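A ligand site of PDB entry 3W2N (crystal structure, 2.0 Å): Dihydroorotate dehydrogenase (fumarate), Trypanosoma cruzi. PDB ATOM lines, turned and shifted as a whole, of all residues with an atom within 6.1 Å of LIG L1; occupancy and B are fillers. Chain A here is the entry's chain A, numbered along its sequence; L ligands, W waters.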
ATOM      1  N   ALA A  20      -1.726   8.307   6.402  1.00  0.00           N
ATOM      2  CA  ALA A  20      -1.272   7.188   5.639  1.00  0.00           C
ATOM      3  C   ALA A  20      -1.207   7.499   4.158  1.00  0.00           C
ATOM      4  O   ALA A  20      -2.097   8.197   3.576  1.00  0.00           O
ATOM      5  CB  ALA A  20      -2.154   5.934   5.891  1.00  0.00           C
ATOM      6  N   LYS A  44       2.648   3.361   4.819  1.00  0.00           N
ATOM      7  CA  LYS A  44       1.735   3.270   3.709  1.00  0.00           C
ATOM      8  C   LYS A  44       0.866   2.016   3.861  1.00  0.00           C
ATOM      9  O   LYS A  44       1.401   0.940   4.079  1.00  0.00           O
ATOM     10  CB  LYS A  44       2.522   3.211   2.414  1.00  0.00           C
ATOM     11  CG  LYS A  44       1.790   2.920   1.141  1.00  0.00           C
ATOM     12  CD  LYS A  44       0.813   3.972   0.721  1.00  0.00           C
ATOM     13  CE  LYS A  44      -0.131   3.541  -0.395  1.00  0.00           C
ATOM     14  NZ  LYS A  44      -1.123   4.634  -0.934  1.00  0.00           N
ATOM     15  N   SER A  45      -0.450   2.156   3.604  1.00  0.00           N
ATOM     16  CA  SER A  45      -1.382   0.998   3.573  1.00  0.00           C
ATOM     17  C   SER A  45      -0.787  -0.053   2.644  1.00  0.00           C
ATOM     18  O   SER A  45      -0.392   0.279   1.525  1.00  0.00           O
ATOM     19  CB  SER A  45      -2.753   1.372   3.089  1.00  0.00           C
ATOM     20  OG  SER A  45      -3.496   2.150   4.058  1.00  0.00           O
ATOM     21  N   THR A  47      -0.600  -4.234   0.964  1.00  0.00           N
ATOM     22  CA  THR A  47      -1.136  -5.505   0.550  1.00  0.00           C
ATOM     23  C   THR A  47      -0.068  -6.564   0.805  1.00  0.00           C
ATOM     24  O   THR A  47       1.114  -6.242   1.015  1.00  0.00           O
ATOM     25  CB  THR A  47      -1.455  -5.468  -0.983  1.00  0.00           C
ATOM     26  OG1 THR A  47      -0.442  -4.766  -1.699  1.00  0.00           O
ATOM     27  CG2 THR A  47      -2.782  -4.790  -1.247  1.00  0.00           C
ATOM     28  N   ARG A  51       2.951  -3.708  -4.874  1.00  0.00           N
ATOM     29  CA  ARG A  51       2.203  -3.090  -5.992  1.00  0.00           C
ATOM     30  C   ARG A  51       2.936  -1.867  -6.561  1.00  0.00           C
ATOM     31  O   ARG A  51       3.498  -1.047  -5.785  1.00  0.00           O
ATOM     32  CB  ARG A  51       0.809  -2.653  -5.541  1.00  0.00           C
ATOM     33  CG  ARG A  51      -0.132  -3.765  -5.136  1.00  0.00           C
ATOM     34  CD  ARG A  51      -1.404  -3.151  -4.508  1.00  0.00           C
ATOM     35  NE  ARG A  51      -2.148  -2.225  -5.407  1.00  0.00           N
ATOM     36  CZ  ARG A  51      -3.135  -2.615  -6.188  1.00  0.00           C
ATOM     37  NH1 ARG A  51      -3.485  -3.889  -6.221  1.00  0.00           N
ATOM     38  NH2 ARG A  51      -3.782  -1.773  -6.929  1.00  0.00           N
ATOM     39  N   ASN A  54      -1.000   2.732  -9.883  1.00  0.00           N
ATOM     40  CA  ASN A  54      -1.504   3.215 -11.200  1.00  0.00           C
ATOM     41  C   ASN A  54      -0.471   3.971 -12.060  1.00  0.00           C
ATOM     42  O   ASN A  54       0.535   4.446 -11.553  1.00  0.00           O
ATOM     43  CB  ASN A  54      -2.764   4.095 -10.995  1.00  0.00           C
ATOM     44  CG  ASN A  54      -3.950   3.330 -10.559  1.00  0.00           C
ATOM     45  OD1 ASN A  54      -4.051   2.109 -10.830  1.00  0.00           O
ATOM     46  ND2 ASN A  54      -4.853   3.991  -9.778  1.00  0.00           N
ATOM     47  N   ASN A  68      -5.897  12.402  -5.881  1.00  0.00           N
ATOM     48  CA  ASN A  68      -5.021  11.272  -6.141  1.00  0.00           C
ATOM     49  C   ASN A  68      -5.828  10.039  -6.559  1.00  0.00           C
ATOM     50  O   ASN A  68      -6.911   9.786  -6.044  1.00  0.00           O
ATOM     51  CB  ASN A  68      -4.095  10.995  -4.952  1.00  0.00           C
ATOM     52  CG  ASN A  68      -4.715  10.076  -3.908  1.00  0.00           C
ATOM     53  OD1 ASN A  68      -4.690   8.836  -4.063  1.00  0.00           O
ATOM     54  ND2 ASN A  68      -5.249  10.670  -2.822  1.00  0.00           N
ATOM     55  N   SER A  69      -5.234   9.256  -7.454  1.00  0.00           N
ATOM     56  CA  SER A  69      -5.661   7.933  -7.626  1.00  0.00           C
ATOM     57  C   SER A  69      -4.406   7.059  -7.745  1.00  0.00           C
ATOM     58  O   SER A  69      -4.032   6.562  -8.813  1.00  0.00           O
ATOM     59  CB  SER A  69      -6.743   7.920  -8.731  1.00  0.00           C
ATOM     60  OG  SER A  69      -6.774   6.622  -9.165  1.00  0.00           O
ATOM     61  N   MET A  70      -3.735   6.867  -6.598  1.00  0.00           N
ATOM     62  CA  MET A  70      -2.416   6.268  -6.620  1.00  0.00           C
ATOM     63  C   MET A  70      -2.485   4.745  -6.986  1.00  0.00           C
ATOM     64  O   MET A  70      -1.511   4.200  -7.583  1.00  0.00           O
ATOM     65  CB  MET A  70      -1.727   6.385  -5.296  1.00  0.00           C
ATOM     66  CG  MET A  70      -1.568   7.748  -4.687  1.00  0.00           C
ATOM     67  SD  MET A  70      -0.518   8.827  -5.621  1.00  0.00           S
ATOM     68  CE  MET A  70       1.081   8.122  -5.364  1.00  0.00           C
ATOM     69  N   GLY A  71      -3.599   4.073  -6.639  1.00  0.00           N
ATOM     70  CA  GLY A  71      -3.744   2.606  -6.870  1.00  0.00           C
ATOM     71  C   GLY A  71      -2.954   1.750  -5.856  1.00  0.00           C
ATOM     72  O   GLY A  71      -2.498   0.636  -6.166  1.00  0.00           O
ATOM     73  N   LEU A  72      -2.705   2.314  -4.675  1.00  0.00           N
ATOM     74  CA  LEU A  72      -1.954   1.680  -3.597  1.00  0.00           C
ATOM     75  C   LEU A  72      -0.620   1.080  -4.032  1.00  0.00           C
ATOM     76  O   LEU A  72      -0.354  -0.089  -3.742  1.00  0.00           O
ATOM     77  CB  LEU A  72      -2.780   0.573  -2.935  1.00  0.00           C
ATOM     78  CG  LEU A  72      -2.322   0.270  -1.483  1.00  0.00           C
ATOM     79  CD1 LEU A  72      -2.921   1.196  -0.439  1.00  0.00           C
ATOM     80  CD2 LEU A  72      -2.765  -1.107  -1.130  1.00  0.00           C
ATOM     81  N   PRO A  73       0.263   1.887  -4.617  1.00  0.00           N
ATOM     82  CA  PRO A  73       1.632   1.419  -4.717  1.00  0.00           C
ATOM     83  C   PRO A  73       2.276   1.183  -3.326  1.00  0.00           C
ATOM     84  O   PRO A  73       2.177   2.054  -2.457  1.00  0.00           O
ATOM     85  CB  PRO A  73       2.345   2.576  -5.446  1.00  0.00           C
ATOM     86  CG  PRO A  73       1.619   3.815  -5.043  1.00  0.00           C
ATOM     87  CD  PRO A  73       0.189   3.358  -4.657  1.00  0.00           C
ATOM     88  N   SER A 100      -4.369  -2.641   4.085  1.00  0.00           N
ATOM     89  CA  SER A 100      -5.510  -2.555   3.236  1.00  0.00           C
ATOM     90  C   SER A 100      -5.620  -3.691   2.195  1.00  0.00           C
ATOM     91  O   SER A 100      -5.470  -3.437   1.048  1.00  0.00           O
ATOM     92  CB  SER A 100      -5.598  -1.183   2.581  1.00  0.00           C
ATOM     93  OG  SER A 100      -6.885  -0.786   2.270  1.00  0.00           O
ATOM     94  N   GLY A 101      -5.886  -4.895   2.627  1.00  0.00           N
ATOM     95  CA  GLY A 101      -5.958  -6.014   1.723  1.00  0.00           C
ATOM     96  C   GLY A 101      -7.159  -5.976   0.797  1.00  0.00           C
ATOM     97  O   GLY A 101      -8.078  -5.289   1.015  1.00  0.00           O
ATOM     98  N   LEU A 102      -7.068  -6.740  -0.268  1.00  0.00           N
ATOM     99  CA  LEU A 102      -8.057  -6.776  -1.299  1.00  0.00           C
ATOM    100  C   LEU A 102      -9.180  -7.771  -1.045  1.00  0.00           C
ATOM    101  O   LEU A 102     -10.058  -7.910  -1.840  1.00  0.00           O
ATOM    102  CB  LEU A 102      -7.392  -7.033  -2.651  1.00  0.00           C
ATOM    103  CG  LEU A 102      -6.611  -5.855  -3.187  1.00  0.00           C
ATOM    104  CD1 LEU A 102      -5.669  -6.217  -4.305  1.00  0.00           C
ATOM    105  CD2 LEU A 102      -7.601  -4.869  -3.679  1.00  0.00           C
ATOM    106  N   ASN A 128      -7.392   0.045   6.962  1.00  0.00           N
ATOM    107  CA  ASN A 128      -7.913   0.990   6.060  1.00  0.00           C
ATOM    108  C   ASN A 128      -9.092   0.359   5.385  1.00  0.00           C
ATOM    109  O   ASN A 128      -8.909  -0.511   4.474  1.00  0.00           O
ATOM    110  CB  ASN A 128      -6.848   1.417   5.073  1.00  0.00           C
ATOM    111  CG  ASN A 128      -7.356   2.261   3.971  1.00  0.00           C
ATOM    112  OD1 ASN A 128      -8.510   2.612   3.893  1.00  0.00           O
ATOM    113  ND2 ASN A 128      -6.470   2.559   3.058  1.00  0.00           N
ATOM    114  N   SER A 130     -11.210   1.658   3.306  1.00  0.00           N
ATOM    115  CA  SER A 130     -11.514   2.139   1.993  1.00  0.00           C
ATOM    116  C   SER A 130     -11.006   1.202   0.910  1.00  0.00           C
ATOM    117  O   SER A 130     -10.989   1.548  -0.177  1.00  0.00           O
ATOM    118  CB  SER A 130     -11.022   3.538   1.807  1.00  0.00           C
ATOM    119  OG  SER A 130     -11.841   4.403   2.446  1.00  0.00           O
ATOM    120  N   CYS A 131     -10.587   0.004   1.265  1.00  0.00           N
ATOM    121  CA  CYS A 131     -10.188  -0.977   0.270  1.00  0.00           C
ATOM    122  C   CYS A 131     -11.394  -1.357  -0.629  1.00  0.00           C
ATOM    123  O   CYS A 131     -12.537  -1.357  -0.250  1.00  0.00           O
ATOM    124  CB  CYS A 131      -9.641  -2.237   0.925  1.00  0.00           C
ATOM    125  SG  CYS A 131     -10.687  -2.750   2.259  1.00  0.00           S
ATOM    126  N   PRO A 132     -10.990  -1.678  -1.926  1.00  0.00           N
ATOM    127  CA  PRO A 132     -12.070  -2.141  -2.786  1.00  0.00           C
ATOM    128  C   PRO A 132     -12.608  -3.486  -2.341  1.00  0.00           C
ATOM    129  O   PRO A 132     -11.921  -4.317  -1.871  1.00  0.00           O
ATOM    130  CB  PRO A 132     -11.379  -2.356  -4.161  1.00  0.00           C
ATOM    131  CG  PRO A 132     -10.187  -1.589  -4.136  1.00  0.00           C
ATOM    132  CD  PRO A 132      -9.705  -1.814  -2.765  1.00  0.00           C
ATOM    133  N   LYS A 165      -9.377   3.221   9.684  1.00  0.00           N
ATOM    134  CA  LYS A 165      -9.401   4.449   8.883  1.00  0.00           C
ATOM    135  C   LYS A 165     -10.671   4.453   8.052  1.00  0.00           C
ATOM    136  O   LYS A 165     -10.979   3.512   7.355  1.00  0.00           O
ATOM    137  CB  LYS A 165      -8.143   4.535   8.044  1.00  0.00           C
ATOM    138  CG  LYS A 165      -8.126   5.678   6.989  1.00  0.00           C
ATOM    139  CD  LYS A 165      -7.658   6.897   7.677  1.00  0.00           C
ATOM    140  CE  LYS A 165      -7.231   7.996   6.703  1.00  0.00           C
ATOM    141  NZ  LYS A 165      -5.958   7.789   6.035  1.00  0.00           N
ATOM    142  N   ASN A 195     -10.376   9.465   5.495  1.00  0.00           N
ATOM    143  CA  ASN A 195      -9.726   9.257   4.212  1.00  0.00           C
ATOM    144  C   ASN A 195     -10.161  10.380   3.216  1.00  0.00           C
ATOM    145  O   ASN A 195     -10.995  11.242   3.502  1.00  0.00           O
ATOM    146  CB  ASN A 195     -10.080   7.881   3.640  1.00  0.00           C
ATOM    147  CG  ASN A 195      -8.945   7.218   2.810  1.00  0.00           C
ATOM    148  OD1 ASN A 195      -8.337   7.826   1.957  1.00  0.00           O
ATOM    149  ND2 ASN A 195      -8.597   5.996   3.148  1.00  0.00           N
ATOM    150  N   SER A 196      -9.567  10.358   2.029  1.00  0.00           N
ATOM    151  CA  SER A 196      -9.902  11.292   0.984  1.00  0.00           C
ATOM    152  C   SER A 196     -11.385  11.311   0.611  1.00  0.00           C
ATOM    153  O   SER A 196     -12.139  10.268   0.735  1.00  0.00           O
ATOM    154  CB  SER A 196      -8.979  11.083  -0.252  1.00  0.00           C
ATOM    155  OG  SER A 196      -9.213   9.796  -0.823  1.00  0.00           O
ATOM    156  N   GLY A 220      -9.520  10.753  -5.238  1.00  0.00           N
ATOM    157  CA  GLY A 220      -9.843  11.225  -3.936  1.00  0.00           C
ATOM    158  C   GLY A 220      -9.271  12.634  -3.684  1.00  0.00           C
ATOM    159  O   GLY A 220      -8.126  12.933  -4.077  1.00  0.00           O
HETATM  160  O1  LIG L   1      -3.550   4.490  -3.002  1.00  0.00           O
HETATM  161  C1  LIG L   1      -4.583   5.156  -3.139  1.00  0.00           C
HETATM  162  O2  LIG L   1      -4.980   5.333  -4.265  1.00  0.00           O
HETATM  163  C2  LIG L   1      -5.304   5.684  -2.014  1.00  0.00           C
HETATM  164  N1  LIG L   1      -5.558   7.074  -1.988  1.00  0.00           N
HETATM  165  C3  LIG L   1      -6.278   7.694  -0.952  1.00  0.00           C
HETATM  166  O3  LIG L   1      -6.509   8.900  -0.912  1.00  0.00           O
HETATM  167  N2  LIG L   1      -6.754   6.822   0.068  1.00  0.00           N
HETATM  168  C4  LIG L   1      -6.592   5.445   0.001  1.00  0.00           C
HETATM  169  O4  LIG L   1      -7.069   4.775   0.920  1.00  0.00           O
HETATM  170  C5  LIG L   1      -5.871   4.846  -1.076  1.00  0.00           C
HETATM  171  C6  LIG L   1      -5.703   3.464  -1.149  1.00  0.00           C
HETATM  172  C7  LIG L   1      -7.118   2.753  -1.462  1.00  0.00           C
HETATM  173  C8  LIG L   1      -6.883   1.316  -1.805  1.00  0.00           C
HETATM  174  C9  LIG L   1      -6.857   0.386  -0.718  1.00  0.00           C
HETATM  175  C10 LIG L   1      -6.592  -1.005  -0.865  1.00  0.00           C
HETATM  176  C11 LIG L   1      -6.423  -1.527  -2.117  1.00  0.00           C
HETATM  177  C12 LIG L   1      -6.457  -0.627  -3.185  1.00  0.00           C
HETATM  178  C13 LIG L   1      -6.699   0.770  -3.071  1.00  0.00           C
HETATM  179  C14 LIG L   1      -6.750   1.554  -4.305  1.00  0.00           C
HETATM  180  F1  LIG L   1      -5.924   2.555  -4.268  1.00  0.00           F
HETATM  181  F2  LIG L   1      -6.469   0.754  -5.464  1.00  0.00           F
HETATM  182  F3  LIG L   1      -8.018   2.109  -4.565  1.00  0.00           F
HETATM  183  N1  LG2 L   2      -5.084   6.854   3.226  1.00  0.00           N
HETATM  184  C1  LG2 L   2      -4.892   5.570   3.623  1.00  0.00           C
HETATM  185  O1  LG2 L   2      -5.531   5.155   4.562  1.00  0.00           O
HETATM  186  N2  LG2 L   2      -4.013   4.739   3.035  1.00  0.00           N
HETATM  187  C2  LG2 L   2      -3.239   5.071   1.991  1.00  0.00           C
HETATM  188  O2  LG2 L   2      -2.353   4.311   1.501  1.00  0.00           O
HETATM  189  C3  LG2 L   2      -3.354   6.445   1.513  1.00  0.00           C
HETATM  190  N3  LG2 L   2      -2.656   6.865   0.476  1.00  0.00           N
HETATM  191  C4  LG2 L   2      -2.648   8.160   0.109  1.00  0.00           C
HETATM  192  C5  LG2 L   2      -1.758   8.623  -0.861  1.00  0.00           C
HETATM  193  C6  LG2 L   2      -1.819   9.988  -1.254  1.00  0.00           C
HETATM  194  C7  LG2 L   2      -0.867  10.463  -2.367  1.00  0.00           C
HETATM  195  C8  LG2 L   2      -2.773  10.895  -0.627  1.00  0.00           C
HETATM  196  C9  LG2 L   2      -2.887  12.332  -1.006  1.00  0.00           C
HETATM  197  C10 LG2 L   2      -3.623  10.455   0.376  1.00  0.00           C
HETATM  198  C11 LG2 L   2      -3.605   9.094   0.745  1.00  0.00           C
HETATM  199  N4  LG2 L   2      -4.473   8.593   1.703  1.00  0.00           N
HETATM  200  C12 LG2 L   2      -4.406   7.297   2.137  1.00  0.00           C
HETATM  201  C13 LG2 L   2      -5.377   9.469   2.411  1.00  0.00           C
HETATM  202  C14 LG2 L   2      -4.714  10.304   3.430  1.00  0.00           C
HETATM  203  O3  LG2 L   2      -4.262   9.446   4.428  1.00  0.00           O
HETATM  204  C15 LG2 L   2      -5.755  11.257   4.068  1.00  0.00           C
HETATM  205  O4  LG2 L   2      -6.779  10.471   4.613  1.00  0.00           O
HETATM  206  C16 LG2 L   2      -6.375  12.241   3.088  1.00  0.00           C
HETATM  207  O5  LG2 L   2      -5.383  12.646   2.120  1.00  0.00           O
HETATM  208  C17 LG2 L   2      -6.937  13.502   3.798  1.00  0.00           C
HETATM  209  O6  LG2 L   2      -6.009  14.270   4.582  1.00  0.00           O
HETATM  210  P1  LG2 L   2      -5.413  15.642   3.954  1.00  0.00           P
HETATM  211  O7  LG2 L   2      -4.447  16.068   4.987  1.00  0.00           O
HETATM  212  O8  LG2 L   2      -6.581  16.539   3.676  1.00  0.00           O
HETATM  213  O9  LG2 L   2      -4.768  15.255   2.642  1.00  0.00           O
HETATM  214  O   HOH W   1      -7.415   5.632  -4.955  1.00  0.00           O
HETATM  215  O   HOH W   2      -8.175   8.201  -3.786  1.00  0.00           O
HETATM  216  O   HOH W   3     -10.296   4.173  -4.234  1.00  0.00           O
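N of Gly 71 sits close to ND2 of Asn 54, at 3.4 Å. The backbone NH (N) of Asn 54 is in hydrogen-bond range of the backbone carbonyl oxygen (O) of Met 70 (2.8 Å). O of Gly 71 lies within hydrogen-bond range of NH2 of Arg 51 (2.8 Å). The backbone carbonyl oxygen (O) of Leu 72 lies within hydrogen-bond range of the guanidinium group (NE) of Arg 51. O of Ser 69 is in hydrogen-bond range of ND2 of Asn 54, at 2.9 Å. The side-chain amide nitrogen of Asn 195 is in hydrogen-bond range of the side-chain amide oxygen of Asn 128. The side-chain amide oxygen (OD1) of Asn 128 sits at hydrogen-bond distance from the backbone NH (N) of Ser 130, 2.9 Å away. The side-chain amide oxygen (OD1) of Asn 68 sits at hydrogen-bond distance from the backbone NH (N) of Met 70 (3.3 Å).
Merely in contact with LIG L1: Arg 51 (3.97 Å), Ser 69 (3.9 Å), Ser 100 (3.2 Å), Leu 102 (3.9 Å), Cys 131 (3.7 Å) and Pro 132 (3.4 Å). Hydrophobic or aromatic side chains within 4 Å of LIG L1: Met 70, Leu 72, Leu 102 and Pro 132. Of the 23 residues printed, 14 come within 4 Å of LIG L1.
ND2 of Asn 128 lies within hydrogen-bond range of O1 of LG2 L2, at 3.1 Å. O4 of LIG L1 lies within hydrogen-bond range of ND2 of Asn 128 (3.1 Å). The backbone NH of Leu 72 is in hydrogen-bond range of an oxygen (O1) of LIG L1, at 2.9 Å. An oxygen (O3) of LIG L1 lies within hydrogen-bond range of the side-chain hydroxyl of Ser 196, 2.8 Å away. The side-chain amino group (NZ) of Lys 165 sits at hydrogen-bond distance from an oxygen (O3) of LG2 L2, at 2.9 Å. N of Ala 20 lies within hydrogen-bond range of O3 of LG2 L2, 3.4 Å away. The backbone NH (N) of Gly 71 is in hydrogen-bond range of an oxygen (O2) of LIG L1. The side-chain amino group (NZ) of Lys 44 is in hydrogen-bond range of an oxygen (O2) of LG2 L2. ND2 of Asn 195 lies within hydrogen-bond range of O1 of LG2 L2, at 3.5 Å. The backbone NH (N) of Met 70 lies within hydrogen-bond range of an oxygen (O2) of LIG L1 (3.1 Å). The side-chain hydroxyl (OG) of Ser 45 lies within hydrogen-bond range of a nitrogen (N2) of LG2 L2 (2.8 Å). O1 of LIG L1 lies within salt-bridge range of NZ of Lys 44, 3.2 Å away. OD1 of Asn 195 lies within hydrogen-bond range of N2 of LIG L1 (2.7 Å). The backbone carbonyl oxygen (O) of Ala 20 lies within hydrogen-bond range of an oxygen (O3) of LG2 L2. The side-chain amide oxygen (OD1) of Asn 68 is in hydrogen-bond range of a nitrogen (N1) of LIG L1, 2.9 Å away.
Water W2 lies within hydrogen-bond range of the backbone carbonyl oxygen of Asn 68 (3.0 Å), the backbone NH of Gly 220 (3.2 Å) and a nitrogen (N1) of LIG L1 (3.4 Å).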
